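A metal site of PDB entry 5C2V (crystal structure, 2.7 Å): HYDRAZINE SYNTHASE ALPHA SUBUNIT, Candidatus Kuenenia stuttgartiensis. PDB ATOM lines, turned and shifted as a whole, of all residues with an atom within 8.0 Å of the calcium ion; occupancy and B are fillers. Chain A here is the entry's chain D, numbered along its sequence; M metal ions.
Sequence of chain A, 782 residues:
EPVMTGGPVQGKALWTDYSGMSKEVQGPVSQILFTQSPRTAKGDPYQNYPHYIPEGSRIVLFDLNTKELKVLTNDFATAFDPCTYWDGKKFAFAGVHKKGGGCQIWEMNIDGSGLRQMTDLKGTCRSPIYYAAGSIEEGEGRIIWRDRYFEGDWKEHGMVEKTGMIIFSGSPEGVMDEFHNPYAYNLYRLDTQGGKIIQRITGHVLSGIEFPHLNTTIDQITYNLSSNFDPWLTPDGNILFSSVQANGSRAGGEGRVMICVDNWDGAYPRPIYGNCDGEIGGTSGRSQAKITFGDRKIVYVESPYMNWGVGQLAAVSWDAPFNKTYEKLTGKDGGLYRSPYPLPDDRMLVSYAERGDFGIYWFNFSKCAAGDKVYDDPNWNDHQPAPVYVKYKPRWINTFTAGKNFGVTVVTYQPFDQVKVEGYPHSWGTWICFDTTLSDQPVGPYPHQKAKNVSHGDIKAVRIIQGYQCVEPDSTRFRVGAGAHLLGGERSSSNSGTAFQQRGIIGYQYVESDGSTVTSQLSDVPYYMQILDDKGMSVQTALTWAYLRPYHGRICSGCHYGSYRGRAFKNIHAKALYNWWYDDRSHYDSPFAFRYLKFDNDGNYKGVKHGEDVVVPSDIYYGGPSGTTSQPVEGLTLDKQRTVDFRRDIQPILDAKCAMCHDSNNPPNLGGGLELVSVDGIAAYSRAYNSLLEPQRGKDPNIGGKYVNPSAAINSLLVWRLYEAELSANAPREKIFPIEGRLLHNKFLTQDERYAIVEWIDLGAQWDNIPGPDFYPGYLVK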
ATOM      1  N   PHE A  34      17.749   7.310  23.490  1.00  0.00           N
ATOM      2  CA  PHE A  34      16.463   7.973  23.304  1.00  0.00           C
ATOM      3  C   PHE A  34      16.159   9.025  24.360  1.00  0.00           C
ATOM      4  O   PHE A  34      16.773   9.069  25.424  1.00  0.00           O
ATOM      5  CB  PHE A  34      15.328   6.931  23.259  1.00  0.00           C
ATOM      6  CG  PHE A  34      15.166   6.134  24.516  1.00  0.00           C
ATOM      7  CD1 PHE A  34      14.307   6.538  25.516  1.00  0.00           C
ATOM      8  CD2 PHE A  34      15.871   4.947  24.691  1.00  0.00           C
ATOM      9  CE1 PHE A  34      14.149   5.793  26.665  1.00  0.00           C
ATOM     10  CE2 PHE A  34      15.726   4.196  25.840  1.00  0.00           C
ATOM     11  CZ  PHE A  34      14.857   4.628  26.836  1.00  0.00           C
ATOM     12  N   GLN A  36      13.699  10.960  27.053  1.00  0.00           N
ATOM     13  CA  GLN A  36      12.586  10.826  27.986  1.00  0.00           C
ATOM     14  C   GLN A  36      12.119  12.208  28.440  1.00  0.00           C
ATOM     15  O   GLN A  36      12.917  12.991  28.951  1.00  0.00           O
ATOM     16  CB  GLN A  36      12.974   9.973  29.193  1.00  0.00           C
ATOM     17  CG  GLN A  36      13.216   8.511  28.882  1.00  0.00           C
ATOM     18  CD  GLN A  36      13.550   7.706  30.115  1.00  0.00           C
ATOM     19  OE1 GLN A  36      14.136   8.226  31.066  1.00  0.00           O
ATOM     20  NE2 GLN A  36      13.182   6.427  30.114  1.00  0.00           N
ATOM     21  N   SER A  37      10.839  12.491  28.255  1.00  0.00           N
ATOM     22  CA  SER A  37      10.273  13.769  28.637  1.00  0.00           C
ATOM     23  C   SER A  37       9.184  13.592  29.686  1.00  0.00           C
ATOM     24  O   SER A  37       8.472  12.588  29.665  1.00  0.00           O
ATOM     25  CB  SER A  37       9.711  14.497  27.406  1.00  0.00           C
ATOM     26  OG  SER A  37      10.735  14.816  26.492  1.00  0.00           O
ATOM     27  N   ARG A  39       5.579  13.853  31.399  1.00  0.00           N
ATOM     28  CA  ARG A  39       4.313  13.910  30.698  1.00  0.00           C
ATOM     29  C   ARG A  39       3.564  15.113  31.241  1.00  0.00           C
ATOM     30  O   ARG A  39       2.955  15.057  32.310  1.00  0.00           O
ATOM     31  CB  ARG A  39       3.502  12.624  30.902  1.00  0.00           C
ATOM     32  CG  ARG A  39       4.312  11.351  30.770  1.00  0.00           C
ATOM     33  CD  ARG A  39       3.549  10.156  31.343  1.00  0.00           C
ATOM     34  NE  ARG A  39       2.199  10.068  30.817  1.00  0.00           N
ATOM     35  CZ  ARG A  39       1.310   9.135  31.180  1.00  0.00           C
ATOM     36  NH1 ARG A  39       1.648   8.219  32.084  1.00  0.00           N
ATOM     37  NH2 ARG A  39       0.102   9.125  30.646  1.00  0.00           N
ATOM     38  N   SER A 351       8.245   5.703  18.217  1.00  0.00           N
ATOM     39  CA  SER A 351       7.691   6.094  19.506  1.00  0.00           C
ATOM     40  C   SER A 351       6.179   6.076  19.403  1.00  0.00           C
ATOM     41  O   SER A 351       5.596   6.712  18.529  1.00  0.00           O
ATOM     42  CB  SER A 351       8.205   7.472  19.931  1.00  0.00           C
ATOM     43  OG  SER A 351       7.620   7.847  21.173  1.00  0.00           O
ATOM     44  N   TYR A 352       5.540   5.342  20.302  1.00  0.00           N
ATOM     45  CA  TYR A 352       4.125   5.044  20.161  1.00  0.00           C
ATOM     46  C   TYR A 352       3.397   5.170  21.494  1.00  0.00           C
ATOM     47  O   TYR A 352       3.852   4.646  22.512  1.00  0.00           O
ATOM     48  CB  TYR A 352       3.956   3.637  19.591  1.00  0.00           C
ATOM     49  CG  TYR A 352       2.549   3.094  19.594  1.00  0.00           C
ATOM     50  CD1 TYR A 352       1.589   3.595  18.737  1.00  0.00           C
ATOM     51  CD2 TYR A 352       2.187   2.045  20.451  1.00  0.00           C
ATOM     52  CE1 TYR A 352       0.296   3.088  18.729  1.00  0.00           C
ATOM     53  CE2 TYR A 352       0.904   1.542  20.452  1.00  0.00           C
ATOM     54  CZ  TYR A 352      -0.030   2.063  19.591  1.00  0.00           C
ATOM     55  OH  TYR A 352      -1.314   1.559  19.582  1.00  0.00           O
ATOM     56  N   ALA A 353       2.278   5.887  21.475  1.00  0.00           N
ATOM     57  CA  ALA A 353       1.365   5.874  22.604  1.00  0.00           C
ATOM     58  C   ALA A 353       0.015   5.349  22.147  1.00  0.00           C
ATOM     59  O   ALA A 353      -0.718   6.038  21.435  1.00  0.00           O
ATOM     60  CB  ALA A 353       1.234   7.268  23.191  1.00  0.00           C
ATOM     61  N   GLY A 356      -1.936   6.637  25.114  1.00  0.00           N
ATOM     62  CA  GLY A 356      -1.329   7.887  25.541  1.00  0.00           C
ATOM     63  C   GLY A 356      -0.060   7.920  26.361  1.00  0.00           C
ATOM     64  O   GLY A 356       0.460   9.007  26.643  1.00  0.00           O
ATOM     65  N   ASP A 357       0.457   6.759  26.754  1.00  0.00           N
ATOM     66  CA  ASP A 357       1.820   6.715  27.287  1.00  0.00           C
ATOM     67  C   ASP A 357       2.793   6.377  26.162  1.00  0.00           C
ATOM     68  O   ASP A 357       2.778   5.261  25.646  1.00  0.00           O
ATOM     69  CB  ASP A 357       1.928   5.697  28.429  1.00  0.00           C
ATOM     70  CG  ASP A 357       3.231   5.840  29.192  1.00  0.00           C
ATOM     71  OD1 ASP A 357       3.683   6.979  29.390  1.00  0.00           O
ATOM     72  OD2 ASP A 357       3.793   4.802  29.596  1.00  0.00           O
ATOM     73  N   PHE A 358       3.631   7.335  25.798  1.00  0.00           N
ATOM     74  CA  PHE A 358       4.592   7.147  24.714  1.00  0.00           C
ATOM     75  C   PHE A 358       5.746   6.245  25.140  1.00  0.00           C
ATOM     76  O   PHE A 358       6.314   6.403  26.222  1.00  0.00           O
ATOM     77  CB  PHE A 358       5.149   8.484  24.223  1.00  0.00           C
ATOM     78  CG  PHE A 358       4.269   9.186  23.223  1.00  0.00           C
ATOM     79  CD1 PHE A 358       4.163   8.712  21.929  1.00  0.00           C
ATOM     80  CD2 PHE A 358       3.558  10.317  23.582  1.00  0.00           C
ATOM     81  CE1 PHE A 358       3.365   9.345  21.005  1.00  0.00           C
ATOM     82  CE2 PHE A 358       2.757  10.959  22.657  1.00  0.00           C
ATOM     83  CZ  PHE A 358       2.654  10.476  21.364  1.00  0.00           C
ATOM     84  N   GLY A 359       6.098   5.295  24.271  1.00  0.00           N
ATOM     85  CA  GLY A 359       7.190   4.376  24.541  1.00  0.00           C
ATOM     86  C   GLY A 359       7.899   3.964  23.267  1.00  0.00           C
ATOM     87  O   GLY A 359       7.442   4.278  22.177  1.00  0.00           O
ATOM     88  N   ILE A 360       9.018   3.251  23.407  1.00  0.00           N
ATOM     89  CA  ILE A 360       9.771   2.804  22.247  1.00  0.00           C
ATOM     90  C   ILE A 360       9.349   1.404  21.821  1.00  0.00           C
ATOM     91  O   ILE A 360       9.300   0.486  22.634  1.00  0.00           O
ATOM     92  CB  ILE A 360      11.289   2.823  22.522  1.00  0.00           C
ATOM     93  CG1 ILE A 360      11.717   4.193  23.033  1.00  0.00           C
ATOM     94  CG2 ILE A 360      12.062   2.445  21.260  1.00  0.00           C
ATOM     95  CD1 ILE A 360      11.407   5.335  22.077  1.00  0.00           C
ATOM     96  N   TYR A 361       9.015   1.247  20.535  1.00  0.00           N
ATOM     97  CA  TYR A 361       8.520  -0.019  20.013  1.00  0.00           C
ATOM     98  C   TYR A 361       9.150  -0.371  18.665  1.00  0.00           C
ATOM     99  O   TYR A 361       9.456   0.507  17.864  1.00  0.00           O
ATOM    100  CB  TYR A 361       6.997   0.018  19.873  1.00  0.00           C
ATOM    101  CG  TYR A 361       6.242   0.247  21.164  1.00  0.00           C
ATOM    102  CD1 TYR A 361       6.033   1.528  21.649  1.00  0.00           C
ATOM    103  CD2 TYR A 361       5.725  -0.816  21.889  1.00  0.00           C
ATOM    104  CE1 TYR A 361       5.336   1.742  22.827  1.00  0.00           C
ATOM    105  CE2 TYR A 361       5.032  -0.612  23.069  1.00  0.00           C
ATOM    106  CZ  TYR A 361       4.840   0.673  23.532  1.00  0.00           C
ATOM    107  OH  TYR A 361       4.143   0.885  24.700  1.00  0.00           O
ATOM    108  N   TYR A 375      11.295  -0.367  25.325  1.00  0.00           N
ATOM    109  CA  TYR A 375      11.262   0.163  26.679  1.00  0.00           C
ATOM    110  C   TYR A 375      10.119   1.170  26.844  1.00  0.00           C
ATOM    111  O   TYR A 375      10.047   2.163  26.118  1.00  0.00           O
ATOM    112  CB  TYR A 375      12.598   0.829  27.017  1.00  0.00           C
ATOM    113  CG  TYR A 375      12.697   1.357  28.426  1.00  0.00           C
ATOM    114  CD1 TYR A 375      12.956   0.508  29.497  1.00  0.00           C
ATOM    115  CD2 TYR A 375      12.538   2.715  28.696  1.00  0.00           C
ATOM    116  CE1 TYR A 375      13.049   0.989  30.792  1.00  0.00           C
ATOM    117  CE2 TYR A 375      12.627   3.203  29.980  1.00  0.00           C
ATOM    118  CZ  TYR A 375      12.879   2.339  31.033  1.00  0.00           C
ATOM    119  OH  TYR A 375      12.968   2.828  32.316  1.00  0.00           O
ATOM    120  N   ASP A 376       9.226   0.908  27.784  1.00  0.00           N
ATOM    121  CA  ASP A 376       8.176   1.868  28.102  1.00  0.00           C
ATOM    122  C   ASP A 376       8.089   2.122  29.608  1.00  0.00           C
ATOM    123  O   ASP A 376       7.718   1.240  30.382  1.00  0.00           O
ATOM    124  CB  ASP A 376       6.817   1.384  27.579  1.00  0.00           C
ATOM    125  CG  ASP A 376       5.720   2.419  27.768  1.00  0.00           C
ATOM    126  OD1 ASP A 376       4.529   2.021  27.761  1.00  0.00           O
ATOM    127  OD2 ASP A 376       6.035   3.615  27.935  1.00  0.00           O
ATOM    128  N   ASP A 377       8.437   3.345  30.001  1.00  0.00           N
ATOM    129  CA  ASP A 377       8.316   3.765  31.386  1.00  0.00           C
ATOM    130  C   ASP A 377       6.993   4.507  31.534  1.00  0.00           C
ATOM    131  O   ASP A 377       6.719   5.429  30.768  1.00  0.00           O
ATOM    132  CB  ASP A 377       9.499   4.662  31.781  1.00  0.00           C
ATOM    133  CG  ASP A 377       9.598   4.894  33.290  1.00  0.00           C
ATOM    134  OD1 ASP A 377       8.577   4.795  33.992  1.00  0.00           O
ATOM    135  OD2 ASP A 377      10.713   5.174  33.772  1.00  0.00           O
ATOM    136  N   PRO A 378       6.161   4.098  32.491  1.00  0.00           N
ATOM    137  CA  PRO A 378       4.887   4.785  32.746  1.00  0.00           C
ATOM    138  C   PRO A 378       5.063   6.233  33.198  1.00  0.00           C
ATOM    139  O   PRO A 378       4.115   7.020  33.110  1.00  0.00           O
ATOM    140  CB  PRO A 378       4.251   3.939  33.851  1.00  0.00           C
ATOM    141  CG  PRO A 378       4.839   2.586  33.670  1.00  0.00           C
ATOM    142  CD  PRO A 378       6.251   2.826  33.233  1.00  0.00           C
ATOM    143  N   ASN A 379       6.252   6.580  33.677  1.00  0.00           N
ATOM    144  CA  ASN A 379       6.500   7.922  34.191  1.00  0.00           C
ATOM    145  C   ASN A 379       7.131   8.873  33.173  1.00  0.00           C
ATOM    146  O   ASN A 379       7.361  10.045  33.468  1.00  0.00           O
ATOM    147  CB  ASN A 379       7.397   7.858  35.428  1.00  0.00           C
ATOM    148  CG  ASN A 379       6.755   7.111  36.581  1.00  0.00           C
ATOM    149  OD1 ASN A 379       5.889   6.267  36.375  1.00  0.00           O
ATOM    150  ND2 ASN A 379       7.166   7.434  37.800  1.00  0.00           N
ATOM    151  N   TRP A 380       7.404   8.366  31.974  1.00  0.00           N
ATOM    152  CA  TRP A 380       8.069   9.179  30.952  1.00  0.00           C
ATOM    153  C   TRP A 380       7.478   8.997  29.552  1.00  0.00           C
ATOM    154  O   TRP A 380       7.089   7.899  29.164  1.00  0.00           O
ATOM    155  CB  TRP A 380       9.561   8.853  30.890  1.00  0.00           C
ATOM    156  CG  TRP A 380      10.325   9.140  32.157  1.00  0.00           C
ATOM    157  CD1 TRP A 380      10.538   8.294  33.199  1.00  0.00           C
ATOM    158  CD2 TRP A 380      10.985  10.365  32.494  1.00  0.00           C
ATOM    159  NE1 TRP A 380      11.285   8.912  34.169  1.00  0.00           N
ATOM    160  CE2 TRP A 380      11.575  10.181  33.762  1.00  0.00           C
ATOM    161  CE3 TRP A 380      11.137  11.602  31.845  1.00  0.00           C
ATOM    162  CZ2 TRP A 380      12.302  11.188  34.398  1.00  0.00           C
ATOM    163  CZ3 TRP A 380      11.857  12.596  32.483  1.00  0.00           C
ATOM    164  CH2 TRP A 380      12.434  12.386  33.745  1.00  0.00           C
ATOM    165  N   ASN A 381       7.415  10.087  28.802  1.00  0.00           N
ATOM    166  CA  ASN A 381       7.204   9.965  27.375  1.00  0.00           C
ATOM    167  C   ASN A 381       8.522   9.558  26.757  1.00  0.00           C
ATOM    168  O   ASN A 381       9.516  10.292  26.840  1.00  0.00           O
ATOM    169  CB  ASN A 381       6.693  11.271  26.760  1.00  0.00           C
ATOM    170  CG  ASN A 381       5.182  11.403  26.849  1.00  0.00           C
ATOM    171  OD1 ASN A 381       4.460  10.412  26.878  1.00  0.00           O
ATOM    172  ND2 ASN A 381       4.699  12.645  26.878  1.00  0.00           N
ATOM    173  N   ASP A 382       8.549   8.382  26.156  1.00  0.00           N
ATOM    174  CA  ASP A 382       9.769   7.814  25.615  1.00  0.00           C
ATOM    175  C   ASP A 382       9.752   7.948  24.102  1.00  0.00           C
ATOM    176  O   ASP A 382       9.003   7.258  23.425  1.00  0.00           O
ATOM    177  CB  ASP A 382       9.911   6.353  26.046  1.00  0.00           C
ATOM    178  CG  ASP A 382       9.763   6.173  27.553  1.00  0.00           C
ATOM    179  OD1 ASP A 382      10.493   6.844  28.305  1.00  0.00           O
ATOM    180  OD2 ASP A 382       8.901   5.373  27.977  1.00  0.00           O
ATOM    181  N   HIS A 383      10.582   8.854  23.585  1.00  0.00           N
ATOM    182  CA  HIS A 383      10.544   9.140  22.154  1.00  0.00           C
ATOM    183  C   HIS A 383      11.926   9.473  21.605  1.00  0.00           C
ATOM    184  O   HIS A 383      12.918   9.455  22.335  1.00  0.00           O
ATOM    185  CB  HIS A 383       9.567  10.285  21.857  1.00  0.00           C
ATOM    186  CG  HIS A 383      10.044  11.624  22.330  1.00  0.00           C
ATOM    187  ND1 HIS A 383      10.264  11.917  23.653  1.00  0.00           N
ATOM    188  CD2 HIS A 383      10.320  12.761  21.648  1.00  0.00           C
ATOM    189  CE1 HIS A 383      10.663  13.167  23.768  1.00  0.00           C
ATOM    190  NE2 HIS A 383      10.702  13.707  22.562  1.00  0.00           N
HETATM  191 CA    CA M   1       6.568   5.854  28.496  1.00  0.00          CA
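OD2 of Asp 357 touches the calcium ion, 3.2 Å away. Within 4 Å of the calcium ion: Asp 357, Phe 358, Asp 376, Asp 377, Trp 380 and Asp 382. Along chain A the residues within 4 Å of the calcium ion span positions 357 to 382. The nearest printed residue that does not touch the calcium ion is Gly 359 (4.3 Å).
The calcium ion is bound by O of Trp 380, O of Asp 377, O of Phe 358, OD2 of Asp 376 and OD2 of Asp 382. The calcium ion has five donor atoms within binding distance.
OD1 of Asp 377 is in hydrogen-bond range of N of Asn 379. The backbone NH (N) of Phe 358 lies close to the side-chain amide oxygen (OD1) of Asn 381 (3.4 Å). OH of Tyr 361 is in hydrogen-bond range of OD1 of Asp 376 (3.3 Å). The side-chain amide nitrogen (NE2) of Gln 36 lies close to the side-chain carboxylate (OD1) of Asp 382. The backbone carbonyl oxygen (O) of Asp 382 sits at hydrogen-bond distance from the side-chain hydroxyl (OG) of Ser 351. The side-chain carboxylate (OD1) of Asp 357 lies within salt-bridge range of the guanidinium group (NH1) of Arg 39 (3.6 Å).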
